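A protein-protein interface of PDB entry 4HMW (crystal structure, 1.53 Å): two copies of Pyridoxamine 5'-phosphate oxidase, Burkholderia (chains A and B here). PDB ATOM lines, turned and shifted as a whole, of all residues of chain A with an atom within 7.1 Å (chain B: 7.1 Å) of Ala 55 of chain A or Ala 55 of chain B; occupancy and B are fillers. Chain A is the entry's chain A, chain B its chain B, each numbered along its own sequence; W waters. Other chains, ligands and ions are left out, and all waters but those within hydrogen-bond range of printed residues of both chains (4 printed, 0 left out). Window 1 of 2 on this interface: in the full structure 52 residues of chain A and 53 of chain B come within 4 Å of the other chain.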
ATOM      1  N   LEU A  52     -12.918  12.473  -5.844  1.00  0.00           N
ATOM      2  CA  LEU A  52     -11.859  11.534  -5.508  1.00  0.00           C
ATOM      3  C   LEU A  52     -11.162  12.022  -4.242  1.00  0.00           C
ATOM      4  O   LEU A  52     -10.774  13.177  -4.169  1.00  0.00           O
ATOM      5  CB  LEU A  52     -10.876  11.519  -6.714  1.00  0.00           C
ATOM      6  CG  LEU A  52      -9.751  10.540  -6.812  1.00  0.00           C
ATOM      7  CD1 LEU A  52     -10.304   9.170  -7.181  1.00  0.00           C
ATOM      8  CD2 LEU A  52      -8.737  11.052  -7.835  1.00  0.00           C
ATOM      9  N   ALA A  53     -11.020  11.168  -3.230  1.00  0.00           N
ATOM     10  CA  ALA A  53     -10.241  11.549  -2.067  1.00  0.00           C
ATOM     11  C   ALA A  53      -8.814  11.241  -2.428  1.00  0.00           C
ATOM     12  O   ALA A  53      -8.450  10.091  -2.529  1.00  0.00           O
ATOM     13  CB  ALA A  53     -10.647  10.733  -0.816  1.00  0.00           C
ATOM     14  N   LEU A  54      -8.012  12.270  -2.636  1.00  0.00           N
ATOM     15  CA  LEU A  54      -6.658  12.112  -3.153  1.00  0.00           C
ATOM     16  C   LEU A  54      -5.659  12.330  -2.039  1.00  0.00           C
ATOM     17  O   LEU A  54      -5.560  13.430  -1.474  1.00  0.00           O
ATOM     18  CB  LEU A  54      -6.391  13.100  -4.323  1.00  0.00           C
ATOM     19  CG  LEU A  54      -5.012  12.916  -4.920  1.00  0.00           C
ATOM     20  CD1 LEU A  54      -5.033  11.708  -5.863  1.00  0.00           C
ATOM     21  CD2 LEU A  54      -4.639  14.145  -5.664  1.00  0.00           C
ATOM     22  N   ALA A  55      -4.912  11.266  -1.741  1.00  0.00           N
ATOM     23  CA  ALA A  55      -3.851  11.313  -0.744  1.00  0.00           C
ATOM     24  C   ALA A  55      -2.506  11.405  -1.432  1.00  0.00           C
ATOM     25  O   ALA A  55      -2.278  10.767  -2.453  1.00  0.00           O
ATOM     26  CB  ALA A  55      -3.881  10.073   0.123  1.00  0.00           C
ATOM     27  N   THR A  56      -1.622  12.196  -0.816  1.00  0.00           N
ATOM     28  CA  THR A  56      -0.255  12.391  -1.260  1.00  0.00           C
ATOM     29  C   THR A  56       0.604  12.413  -0.001  1.00  0.00           C
ATOM     30  O   THR A  56       0.082  12.427   1.129  1.00  0.00           O
ATOM     31  CB  THR A  56      -0.116  13.731  -2.065  1.00  0.00           C
ATOM     32  OG1 THR A  56      -0.530  14.833  -1.240  1.00  0.00           O
ATOM     33  CG2 THR A  56      -0.953  13.707  -3.347  1.00  0.00           C
ATOM     34  N   ALA A  57       1.915  12.377  -0.169  1.00  0.00           N
ATOM     35  CA  ALA A  57       2.812  12.405   0.972  1.00  0.00           C
ATOM     36  C   ALA A  57       4.065  13.196   0.708  1.00  0.00           C
ATOM     37  O   ALA A  57       4.534  13.317  -0.432  1.00  0.00           O
ATOM     38  CB  ALA A  57       3.169  11.010   1.406  1.00  0.00           C
ATOM     39  N   ILE A  63       1.281  12.006   5.492  1.00  0.00           N
ATOM     40  CA  ILE A  63       0.308  11.914   4.417  1.00  0.00           C
ATOM     41  C   ILE A  63      -0.733  13.030   4.584  1.00  0.00           C
ATOM     42  O   ILE A  63      -1.113  13.380   5.723  1.00  0.00           O
ATOM     43  CB  ILE A  63      -0.401  10.556   4.457  1.00  0.00           C
ATOM     44  CG1 ILE A  63       0.639   9.428   4.408  1.00  0.00           C
ATOM     45  CG2 ILE A  63      -1.401  10.443   3.340  1.00  0.00           C
ATOM     46  CD1 ILE A  63       0.059   8.032   4.583  1.00  0.00           C
ATOM     47  N   SER A  64      -1.148  13.604   3.451  1.00  0.00           N
ATOM     48  CA  SER A  64      -2.230  14.593   3.415  1.00  0.00           C
ATOM     49  C   SER A  64      -3.312  14.156   2.429  1.00  0.00           C
ATOM     50  O   SER A  64      -3.077  13.306   1.585  1.00  0.00           O
ATOM     51  CB  SER A  64      -1.661  15.961   2.992  1.00  0.00           C
ATOM     52  OG  SER A  64      -1.112  15.860   1.678  1.00  0.00           O
ATOM     53  N   SER A  65      -4.506  14.730   2.541  1.00  0.00           N
ATOM     54  CA  SER A  65      -5.636  14.348   1.705  1.00  0.00           C
ATOM     55  C   SER A  65      -6.521  15.543   1.374  1.00  0.00           C
ATOM     56  O   SER A  65      -6.592  16.484   2.156  1.00  0.00           O
ATOM     57  CB  SER A  65      -6.526  13.294   2.386  1.00  0.00           C
ATOM     58  OG  SER A  65      -5.811  12.162   2.778  1.00  0.00           O
ATOM     59  N   ARG A  66      -7.205  15.479   0.228  1.00  0.00           N
ATOM     60  CA  ARG A  66      -8.210  16.478  -0.152  1.00  0.00           C
ATOM     61  C   ARG A  66      -9.069  15.900  -1.255  1.00  0.00           C
ATOM     62  O   ARG A  66      -8.628  14.998  -1.994  1.00  0.00           O
ATOM     63  CB  ARG A  66      -7.582  17.797  -0.640  1.00  0.00           C
ATOM     64  CG  ARG A  66      -6.908  17.756  -1.993  1.00  0.00           C
ATOM     65  CD  ARG A  66      -5.733  16.828  -2.002  1.00  0.00           C
ATOM     66  NE  ARG A  66      -4.665  17.363  -1.234  1.00  0.00           N
ATOM     67  CZ  ARG A  66      -3.578  16.681  -0.862  1.00  0.00           C
ATOM     68  NH1 ARG A  66      -2.638  17.310  -0.195  1.00  0.00           N
ATOM     69  NH2 ARG A  66      -3.418  15.383  -1.151  1.00  0.00           N
ATOM     70  N   GLU A  91       4.025  18.064  -2.883  1.00  0.00           N
ATOM     71  CA  GLU A  91       4.184  16.662  -2.484  1.00  0.00           C
ATOM     72  C   GLU A  91       4.275  15.748  -3.711  1.00  0.00           C
ATOM     73  O   GLU A  91       5.080  14.828  -3.737  1.00  0.00           O
ATOM     74  CB  GLU A  91       3.045  16.233  -1.539  1.00  0.00           C
ATOM     75  CG  GLU A  91       3.277  16.737  -0.132  1.00  0.00           C
ATOM     76  CD  GLU A  91       2.165  16.480   0.886  1.00  0.00           C
ATOM     77  OE1 GLU A  91       1.246  15.644   0.645  1.00  0.00           O
ATOM     78  OE2 GLU A  91       2.243  17.117   1.979  1.00  0.00           O
ATOM     79  N   LEU A  92       3.466  16.018  -4.741  1.00  0.00           N
ATOM     80  CA  LEU A  92       3.533  15.272  -5.981  1.00  0.00           C
ATOM     81  C   LEU A  92       4.920  15.416  -6.635  1.00  0.00           C
ATOM     82  O   LEU A  92       5.469  14.452  -7.183  1.00  0.00           O
ATOM     83  CB  LEU A  92       2.444  15.744  -6.956  1.00  0.00           C
ATOM     84  CG  LEU A  92       1.026  15.320  -6.516  1.00  0.00           C
ATOM     85  CD1 LEU A  92       0.015  15.910  -7.478  1.00  0.00           C
ATOM     86  CD2 LEU A  92       0.881  13.794  -6.401  1.00  0.00           C
ATOM     87  N   TRP A  97       3.980   9.765  -5.464  1.00  0.00           N
ATOM     88  CA  TRP A  97       2.978   8.770  -5.118  1.00  0.00           C
ATOM     89  C   TRP A  97       1.644   9.418  -4.806  1.00  0.00           C
ATOM     90  O   TRP A  97       1.569  10.506  -4.237  1.00  0.00           O
ATOM     91  CB  TRP A  97       3.444   7.923  -3.934  1.00  0.00           C
ATOM     92  CG  TRP A  97       4.634   7.027  -4.239  1.00  0.00           C
ATOM     93  CD1 TRP A  97       5.868   7.043  -3.633  1.00  0.00           C
ATOM     94  CD2 TRP A  97       4.683   5.984  -5.218  1.00  0.00           C
ATOM     95  NE1 TRP A  97       6.676   6.063  -4.175  1.00  0.00           N
ATOM     96  CE2 TRP A  97       5.971   5.403  -5.156  1.00  0.00           C
ATOM     97  CE3 TRP A  97       3.757   5.476  -6.140  1.00  0.00           C
ATOM     98  CZ2 TRP A  97       6.353   4.338  -5.984  1.00  0.00           C
ATOM     99  CZ3 TRP A  97       4.131   4.425  -6.960  1.00  0.00           C
ATOM    100  CH2 TRP A  97       5.420   3.868  -6.879  1.00  0.00           C
ATOM    101  N   ALA A  98       0.573   8.762  -5.208  1.00  0.00           N
ATOM    102  CA  ALA A  98      -0.745   9.252  -4.866  1.00  0.00           C
ATOM    103  C   ALA A  98      -1.715   8.093  -4.806  1.00  0.00           C
ATOM    104  O   ALA A  98      -1.492   7.057  -5.433  1.00  0.00           O
ATOM    105  CB  ALA A  98      -1.189  10.263  -5.899  1.00  0.00           C
ATOM    106  N   SER A  99      -2.790   8.268  -4.040  1.00  0.00           N
ATOM    107  CA  SER A  99      -3.832   7.268  -3.970  1.00  0.00           C
ATOM    108  C   SER A  99      -5.132   8.024  -3.970  1.00  0.00           C
ATOM    109  O   SER A  99      -5.347   8.895  -3.137  1.00  0.00           O
ATOM    110  CB  SER A  99      -3.690   6.407  -2.711  1.00  0.00           C
ATOM    111  OG  SER A  99      -4.715   5.428  -2.615  1.00  0.00           O
ATOM    112  N   GLY A 100      -5.987   7.669  -4.920  1.00  0.00           N
ATOM    113  CA  GLY A 100      -7.297   8.276  -5.031  1.00  0.00           C
ATOM    114  C   GLY A 100      -8.402   7.285  -4.713  1.00  0.00           C
ATOM    115  O   GLY A 100      -8.361   6.132  -5.133  1.00  0.00           O
ATOM    116  N   LEU A 101      -9.394   7.735  -3.947  1.00  0.00           N
ATOM    117  CA  LEU A 101     -10.490   6.853  -3.542  1.00  0.00           C
ATOM    118  C   LEU A 101     -11.850   7.432  -3.928  1.00  0.00           C
ATOM    119  O   LEU A 101     -12.188   8.540  -3.569  1.00  0.00           O
ATOM    120  CB  LEU A 101     -10.424   6.597  -2.036  1.00  0.00           C
ATOM    121  CG  LEU A 101     -11.426   5.625  -1.443  1.00  0.00           C
ATOM    122  CD1 LEU A 101     -11.130   4.186  -1.892  1.00  0.00           C
ATOM    123  CD2 LEU A 101     -11.464   5.759   0.083  1.00  0.00           C
ATOM    124  N   LEU B  52     -14.884   7.815   6.426  1.00  0.00           N
ATOM    125  CA  LEU B  52     -13.600   8.457   6.383  1.00  0.00           C
ATOM    126  C   LEU B  52     -12.717   7.767   5.331  1.00  0.00           C
ATOM    127  O   LEU B  52     -12.527   6.533   5.365  1.00  0.00           O
ATOM    128  CB  LEU B  52     -12.968   8.288   7.780  1.00  0.00           C
ATOM    129  CG  LEU B  52     -11.612   8.958   8.056  1.00  0.00           C
ATOM    130  CD1 LEU B  52     -11.797  10.448   8.200  1.00  0.00           C
ATOM    131  CD2 LEU B  52     -10.944   8.379   9.289  1.00  0.00           C
ATOM    132  N   ALA B  53     -12.192   8.535   4.386  1.00  0.00           N
ATOM    133  CA  ALA B  53     -11.222   7.987   3.445  1.00  0.00           C
ATOM    134  C   ALA B  53      -9.862   7.955   4.118  1.00  0.00           C
ATOM    135  O   ALA B  53      -9.236   8.995   4.291  1.00  0.00           O
ATOM    136  CB  ALA B  53     -11.185   8.836   2.201  1.00  0.00           C
ATOM    137  N   LEU B  54      -9.453   6.756   4.563  1.00  0.00           N
ATOM    138  CA  LEU B  54      -8.215   6.576   5.328  1.00  0.00           C
ATOM    139  C   LEU B  54      -7.046   6.137   4.453  1.00  0.00           C
ATOM    140  O   LEU B  54      -7.090   5.059   3.861  1.00  0.00           O
ATOM    141  CB  LEU B  54      -8.419   5.531   6.440  1.00  0.00           C
ATOM    142  CG  LEU B  54      -7.223   5.346   7.384  1.00  0.00           C
ATOM    143  CD1 LEU B  54      -7.045   6.523   8.290  1.00  0.00           C
ATOM    144  CD2 LEU B  54      -7.408   4.105   8.194  1.00  0.00           C
ATOM    145  N   ALA B  55      -6.001   6.953   4.420  1.00  0.00           N
ATOM    146  CA  ALA B  55      -4.787   6.687   3.638  1.00  0.00           C
ATOM    147  C   ALA B  55      -3.637   6.322   4.561  1.00  0.00           C
ATOM    148  O   ALA B  55      -3.446   6.941   5.612  1.00  0.00           O
ATOM    149  CB  ALA B  55      -4.431   7.906   2.827  1.00  0.00           C
ATOM    150  N   THR B  56      -2.898   5.299   4.141  1.00  0.00           N
ATOM    151  CA  THR B  56      -1.740   4.784   4.856  1.00  0.00           C
ATOM    152  C   THR B  56      -0.659   4.526   3.774  1.00  0.00           C
ATOM    153  O   THR B  56      -0.939   4.536   2.591  1.00  0.00           O
ATOM    154  CB  THR B  56      -2.059   3.481   5.600  1.00  0.00           C
ATOM    155  OG1 THR B  56      -2.651   2.541   4.706  1.00  0.00           O
ATOM    156  CG2 THR B  56      -3.004   3.749   6.766  1.00  0.00           C
ATOM    157  N   ALA B  57       0.579   4.300   4.193  1.00  0.00           N
ATOM    158  CA  ALA B  57       1.649   4.020   3.248  1.00  0.00           C
ATOM    159  C   ALA B  57       2.574   2.913   3.704  1.00  0.00           C
ATOM    160  O   ALA B  57       2.747   2.644   4.903  1.00  0.00           O
ATOM    161  CB  ALA B  57       2.424   5.261   2.929  1.00  0.00           C
ATOM    162  N   ILE B  63       1.194   4.692  -1.389  1.00  0.00           N
ATOM    163  CA  ILE B  63       0.054   5.021  -0.561  1.00  0.00           C
ATOM    164  C   ILE B  63      -1.143   4.163  -0.974  1.00  0.00           C
ATOM    165  O   ILE B  63      -1.318   3.865  -2.149  1.00  0.00           O
ATOM    166  CB  ILE B  63      -0.327   6.484  -0.737  1.00  0.00           C
ATOM    167  CG1 ILE B  63       0.881   7.381  -0.544  1.00  0.00           C
ATOM    168  CG2 ILE B  63      -1.471   6.860   0.212  1.00  0.00           C
ATOM    169  CD1 ILE B  63       0.582   8.847  -0.731  1.00  0.00           C
ATOM    170  N   SER B  64      -1.931   3.739   0.011  1.00  0.00           N
ATOM    171  CA  SER B  64      -3.176   3.033  -0.224  1.00  0.00           C
ATOM    172  C   SER B  64      -4.295   3.717   0.585  1.00  0.00           C
ATOM    173  O   SER B  64      -4.032   4.481   1.500  1.00  0.00           O
ATOM    174  CB  SER B  64      -3.042   1.566   0.181  1.00  0.00           C
ATOM    175  OG  SER B  64      -2.843   1.473   1.571  1.00  0.00           O
ATOM    176  N   SER B  65      -5.534   3.484   0.186  1.00  0.00           N
ATOM    177  CA  SER B  65      -6.668   4.134   0.819  1.00  0.00           C
ATOM    178  C   SER B  65      -7.908   3.244   0.764  1.00  0.00           C
ATOM    179  O   SER B  65      -8.024   2.372  -0.076  1.00  0.00           O
ATOM    180  CB  SER B  65      -6.931   5.534   0.228  1.00  0.00           C
ATOM    181  OG  SER B  65      -7.093   5.513  -1.166  1.00  0.00           O
ATOM    182  N   ARG B  66      -8.802   3.473   1.711  1.00  0.00           N
ATOM    183  CA  ARG B  66     -10.069   2.774   1.813  1.00  0.00           C
ATOM    184  C   ARG B  66     -10.981   3.539   2.760  1.00  0.00           C
ATOM    185  O   ARG B  66     -10.526   4.345   3.593  1.00  0.00           O
ATOM    186  CB  ARG B  66      -9.869   1.343   2.342  1.00  0.00           C
ATOM    187  CG  ARG B  66      -9.573   1.234   3.843  1.00  0.00           C
ATOM    188  CD  ARG B  66      -8.252   1.808   4.223  1.00  0.00           C
ATOM    189  NE  ARG B  66      -7.158   1.052   3.666  1.00  0.00           N
ATOM    190  CZ  ARG B  66      -5.883   1.433   3.626  1.00  0.00           C
ATOM    191  NH1 ARG B  66      -5.472   2.623   4.005  1.00  0.00           N
ATOM    192  NH2 ARG B  66      -4.986   0.588   3.184  1.00  0.00           N
ATOM    193  N   LYS B  88      -4.086  -2.117   5.646  1.00  0.00           N
ATOM    194  CA  LYS B  88      -3.937  -0.870   6.396  1.00  0.00           C
ATOM    195  C   LYS B  88      -3.218  -1.152   7.712  1.00  0.00           C
ATOM    196  O   LYS B  88      -2.431  -0.336   8.190  1.00  0.00           O
ATOM    197  CB  LYS B  88      -5.285  -0.203   6.628  1.00  0.00           C
ATOM    198  CG  LYS B  88      -6.009  -0.629   7.878  1.00  0.00           C
ATOM    199  CD  LYS B  88      -7.461  -0.178   7.859  1.00  0.00           C
ATOM    200  CE  LYS B  88      -8.270  -0.842   6.748  1.00  0.00           C
ATOM    201  NZ  LYS B  88      -8.289  -2.340   6.858  1.00  0.00           N
ATOM    202  N   GLU B  91       0.438  -1.551   7.153  1.00  0.00           N
ATOM    203  CA  GLU B  91       1.062  -0.260   6.814  1.00  0.00           C
ATOM    204  C   GLU B  91       1.179   0.644   8.051  1.00  0.00           C
ATOM    205  O   GLU B  91       2.209   1.313   8.245  1.00  0.00           O
ATOM    206  CB  GLU B  91       0.317   0.421   5.642  1.00  0.00           C
ATOM    207  CG  GLU B  91       0.606  -0.329   4.316  1.00  0.00           C
ATOM    208  CD  GLU B  91      -0.062   0.204   3.054  1.00  0.00           C
ATOM    209  OE1 GLU B  91      -0.729   1.254   3.095  1.00  0.00           O
ATOM    210  OE2 GLU B  91       0.106  -0.463   1.992  1.00  0.00           O
ATOM    211  N   LEU B  92       0.133   0.679   8.879  1.00  0.00           N
ATOM    212  CA  LEU B  92       0.183   1.441  10.117  1.00  0.00           C
ATOM    213  C   LEU B  92       1.313   0.969  11.021  1.00  0.00           C
ATOM    214  O   LEU B  92       1.984   1.777  11.642  1.00  0.00           O
ATOM    215  CB  LEU B  92      -1.138   1.326  10.869  1.00  0.00           C
ATOM    216  CG  LEU B  92      -2.252   2.145  10.205  1.00  0.00           C
ATOM    217  CD1 LEU B  92      -3.606   1.847  10.847  1.00  0.00           C
ATOM    218  CD2 LEU B  92      -1.944   3.624  10.299  1.00  0.00           C
ATOM    219  N   TRP B  97       2.214   6.889  10.094  1.00  0.00           N
ATOM    220  CA  TRP B  97       1.489   8.057   9.599  1.00  0.00           C
ATOM    221  C   TRP B  97       0.198   7.631   8.896  1.00  0.00           C
ATOM    222  O   TRP B  97       0.141   6.596   8.201  1.00  0.00           O
ATOM    223  CB  TRP B  97       2.354   8.858   8.633  1.00  0.00           C
ATOM    224  CG  TRP B  97       3.675   9.371   9.122  1.00  0.00           C
ATOM    225  CD1 TRP B  97       4.904   8.944   8.681  1.00  0.00           C
ATOM    226  CD2 TRP B  97       3.938  10.395  10.104  1.00  0.00           C
ATOM    227  NE1 TRP B  97       5.902   9.653   9.307  1.00  0.00           N
ATOM    228  CE2 TRP B  97       5.345  10.534  10.195  1.00  0.00           C
ATOM    229  CE3 TRP B  97       3.136  11.209  10.906  1.00  0.00           C
ATOM    230  CZ2 TRP B  97       5.958  11.460  11.052  1.00  0.00           C
ATOM    231  CZ3 TRP B  97       3.752  12.132  11.768  1.00  0.00           C
ATOM    232  CH2 TRP B  97       5.149  12.227  11.842  1.00  0.00           C
ATOM    233  N   ALA B  98      -0.850   8.424   9.086  1.00  0.00           N
ATOM    234  CA  ALA B  98      -2.102   8.212   8.370  1.00  0.00           C
ATOM    235  C   ALA B  98      -2.800   9.537   8.144  1.00  0.00           C
ATOM    236  O   ALA B  98      -2.568  10.526   8.857  1.00  0.00           O
ATOM    237  CB  ALA B  98      -3.004   7.289   9.113  1.00  0.00           C
ATOM    238  N   SER B  99      -3.718   9.537   7.187  1.00  0.00           N
ATOM    239  CA  SER B  99      -4.531  10.730   6.944  1.00  0.00           C
ATOM    240  C   SER B  99      -5.935  10.275   6.661  1.00  0.00           C
ATOM    241  O   SER B  99      -6.134   9.308   5.947  1.00  0.00           O
ATOM    242  CB  SER B  99      -3.979  11.507   5.750  1.00  0.00           C
ATOM    243  OG  SER B  99      -4.747  12.676   5.529  1.00  0.00           O
ATOM    244  N   GLY B 100      -6.908  10.971   7.227  1.00  0.00           N
ATOM    245  CA  GLY B 100      -8.295  10.650   6.974  1.00  0.00           C
ATOM    246  C   GLY B 100      -9.018  11.850   6.396  1.00  0.00           C
ATOM    247  O   GLY B 100      -8.743  12.951   6.796  1.00  0.00           O
ATOM    248  N   LEU B 101      -9.940  11.622   5.457  1.00  0.00           N
ATOM    249  CA  LEU B 101     -10.680  12.715   4.843  1.00  0.00           C
ATOM    250  C   LEU B 101     -12.167  12.442   4.950  1.00  0.00           C
ATOM    251  O   LEU B 101     -12.638  11.374   4.559  1.00  0.00           O
ATOM    252  CB  LEU B 101     -10.268  12.853   3.363  1.00  0.00           C
ATOM    253  CG  LEU B 101     -10.894  14.046   2.616  1.00  0.00           C
ATOM    254  CD1 LEU B 101     -10.329  15.333   3.179  1.00  0.00           C
ATOM    255  CD2 LEU B 101     -10.632  13.943   1.100  1.00  0.00           C
ATOM    256  N   LEU B 180      -6.722   7.657  15.746  1.00  0.00           N
ATOM    257  CA  LEU B 180      -6.037   8.549  14.864  1.00  0.00           C
ATOM    258  C   LEU B 180      -5.901   9.866  15.583  1.00  0.00           C
ATOM    259  O   LEU B 180      -6.873  10.572  15.752  1.00  0.00           O
ATOM    260  CB  LEU B 180      -6.787   8.677  13.540  1.00  0.00           C
ATOM    261  CG  LEU B 180      -6.205   9.631  12.489  1.00  0.00           C
ATOM    262  CD1 LEU B 180      -4.783   9.252  12.145  1.00  0.00           C
ATOM    263  CD2 LEU B 180      -7.082   9.674  11.232  1.00  0.00           C
HETATM  264  O   HOH W   1      -7.561  10.098   2.204  1.00  0.00           O
HETATM  265  O   HOH W   2       0.233  11.945   8.298  1.00  0.00           O
HETATM  266  O   HOH W   3      -7.533   8.602  -0.159  1.00  0.00           O
HETATM  267  O   HOH W   4       0.662   5.119  -4.229  1.00  0.00           O
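Ala 53 of chain A touches Leu 101 of chain B, and with the chains exchanged Leu 101 of chain A touches Ala 53 of chain B.
Ala 55 of chain A touches Ile 63 of chain B, and with the chains exchanged Ile 63 of chain A touches Ala 55 of chain B.
Ala 57 of chain A touches Ile 63 of chain B, and with the chains exchanged Ile 63 of chain A touches Ala 57 of chain B.
Ser 64 of chain A touches Ser 99 of chain B, and with the chains exchanged Ser 99 of chain A touches Ser 64 of chain B.
Of the 21 pairs that touch across the chains among the printed residues, 20 have their exchanged pair printed and touching as well.
The backbone carbonyl oxygen (O) of Arg 66 of chain A sits at hydrogen-bond distance from the backbone NH (N) of Leu 54 of chain A (2.9 Å).
The side-chain carboxylate of Glu 91 of chain A sits at hydrogen-bond distance from the side-chain hydroxyl of Thr 56 of chain A.
The side-chain hydroxyl (OG) of Ser 64 of chain A sits at hydrogen-bond distance from the guanidinium group (NH1) of Arg 66 of chain A, 2.8 Å away.
The backbone NH (N) of Ala 55 of chain B is in hydrogen-bond range of the backbone carbonyl oxygen (O) of Ser 99 of chain B, 2.8 Å away.
The guanidinium group of Arg 66 of chain B lies within hydrogen-bond range of the side-chain hydroxyl of Ser 64 of chain B, 2.8 Å away.
The guanidinium group (NH2) of Arg 66 of chain A lies within hydrogen-bond range of the side-chain hydroxyl (OG1) of Thr 56 of chain A, 2.9 Å away.
OG of Ser 99 of chain A sits at hydrogen-bond distance from OG of Ser 65 of chain B (2.8 Å).
OG of Ser 65 of chain A is in hydrogen-bond range of OG of Ser 99 of chain B (3.0 Å).
Water W1 bridges OG of Ser 65 of chain A (2.8 Å) and O of Ala 53 of chain B (2.9 Å).
Water W4 lies within hydrogen-bond range of the backbone NH (N) of Ile 63 of chain B (2.9 Å) and the backbone carbonyl oxygen (O) of Ala 98 of chain A (3.1 Å).
Water W3 lies within hydrogen-bond range of the backbone carbonyl oxygen (O) of Ala 53 of chain A (2.9 Å) and the side-chain hydroxyl (OG) of Ser 65 of chain B (3.3 Å).
Water W2 lies within hydrogen-bond range of N of Ile 63 of chain A (3.0 Å) and O of Ala 98 of chain B (3.2 Å).
Printed residues of chain B within 4 Å of Ala 55 of chain A: Ala 55 and Ile 63.
Ala 55 of chain B touches just these residues of chain A: Ala 55 (3.5 Å) and Ile 63 (3.8 Å).
Of the printed residues of chain A, Ala 57 of chain B touches Ile 63.
Of the printed residues of chain A, Ser 65 of chain B touches Ser 99 (2.8 Å) and Leu 101 (3.6 Å).
Printed residues of chain B within 4 Å of Thr 56 of chain A: Ile 63.
Of the printed residues of chain B, Ser 64 of chain A touches Ser 99.
Printed residues of chain B within 4 Å of Ser 65 of chain A: Ser 99 and Leu 101.
The nearest printed residue of chain B that does not touch Ala 55 of chain A is Ser 65 of chain B (5.5 Å).
Among the printed residues, pairs that only touch across the chains: Ile 63 of chain A with Ser 99 of chain B (3.4 Å), Arg 66 of chain A with Leu 101 of chain B (3.4 Å), Ala 55 of chain A with Ala 55 of chain B (3.5 Å), Leu 101 of chain A with Arg 66 of chain B (3.5 Å), Ser 99 of chain A with Ile 63 of chain B (3.5 Å), Ala 53 of chain A with Ala 53 of chain B (3.6 Å), Leu 101 of chain A with Ser 65 of chain B (3.6 Å), Thr 56 of chain A with Ile 63 of chain B (3.6 Å), Ser 99 of chain A with Ser 64 of chain B (3.7 Å), Ile 63 of chain A with Thr 56 of chain B (3.7 Å), Ser 64 of chain A with Ser 99 of chain B (3.7 Å), Ala 53 of chain A with Leu 101 of chain B (3.7 Å), Leu 101 of chain A with Ala 53 of chain B (3.7 Å), Ile 63 of chain A with Ala 57 of chain B (3.8 Å), Ile 63 of chain A with Ala 55 of chain B (3.8 Å), Ala 57 of chain A with Ile 63 of chain B (3.8 Å), Ala 55 of chain A with Ile 63 of chain B (3.9 Å), Ser 65 of chain A with Leu 101 of chain B (3.9 Å) and Ile 63 of chain A with Trp 97 of chain B (3.9 Å).
Hydrophobic or aromatic side chains of chain A that line the printed part of chain B: Ala 53, Ala 55, Ala 57, Ile 63 and Leu 101.
Among the printed residues, 21 pairs touch across the chains.
Among the printed residues, no Asp or Glu carboxylate lies within 4 Å of a Lys or Arg side-chain nitrogen of the other chain.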
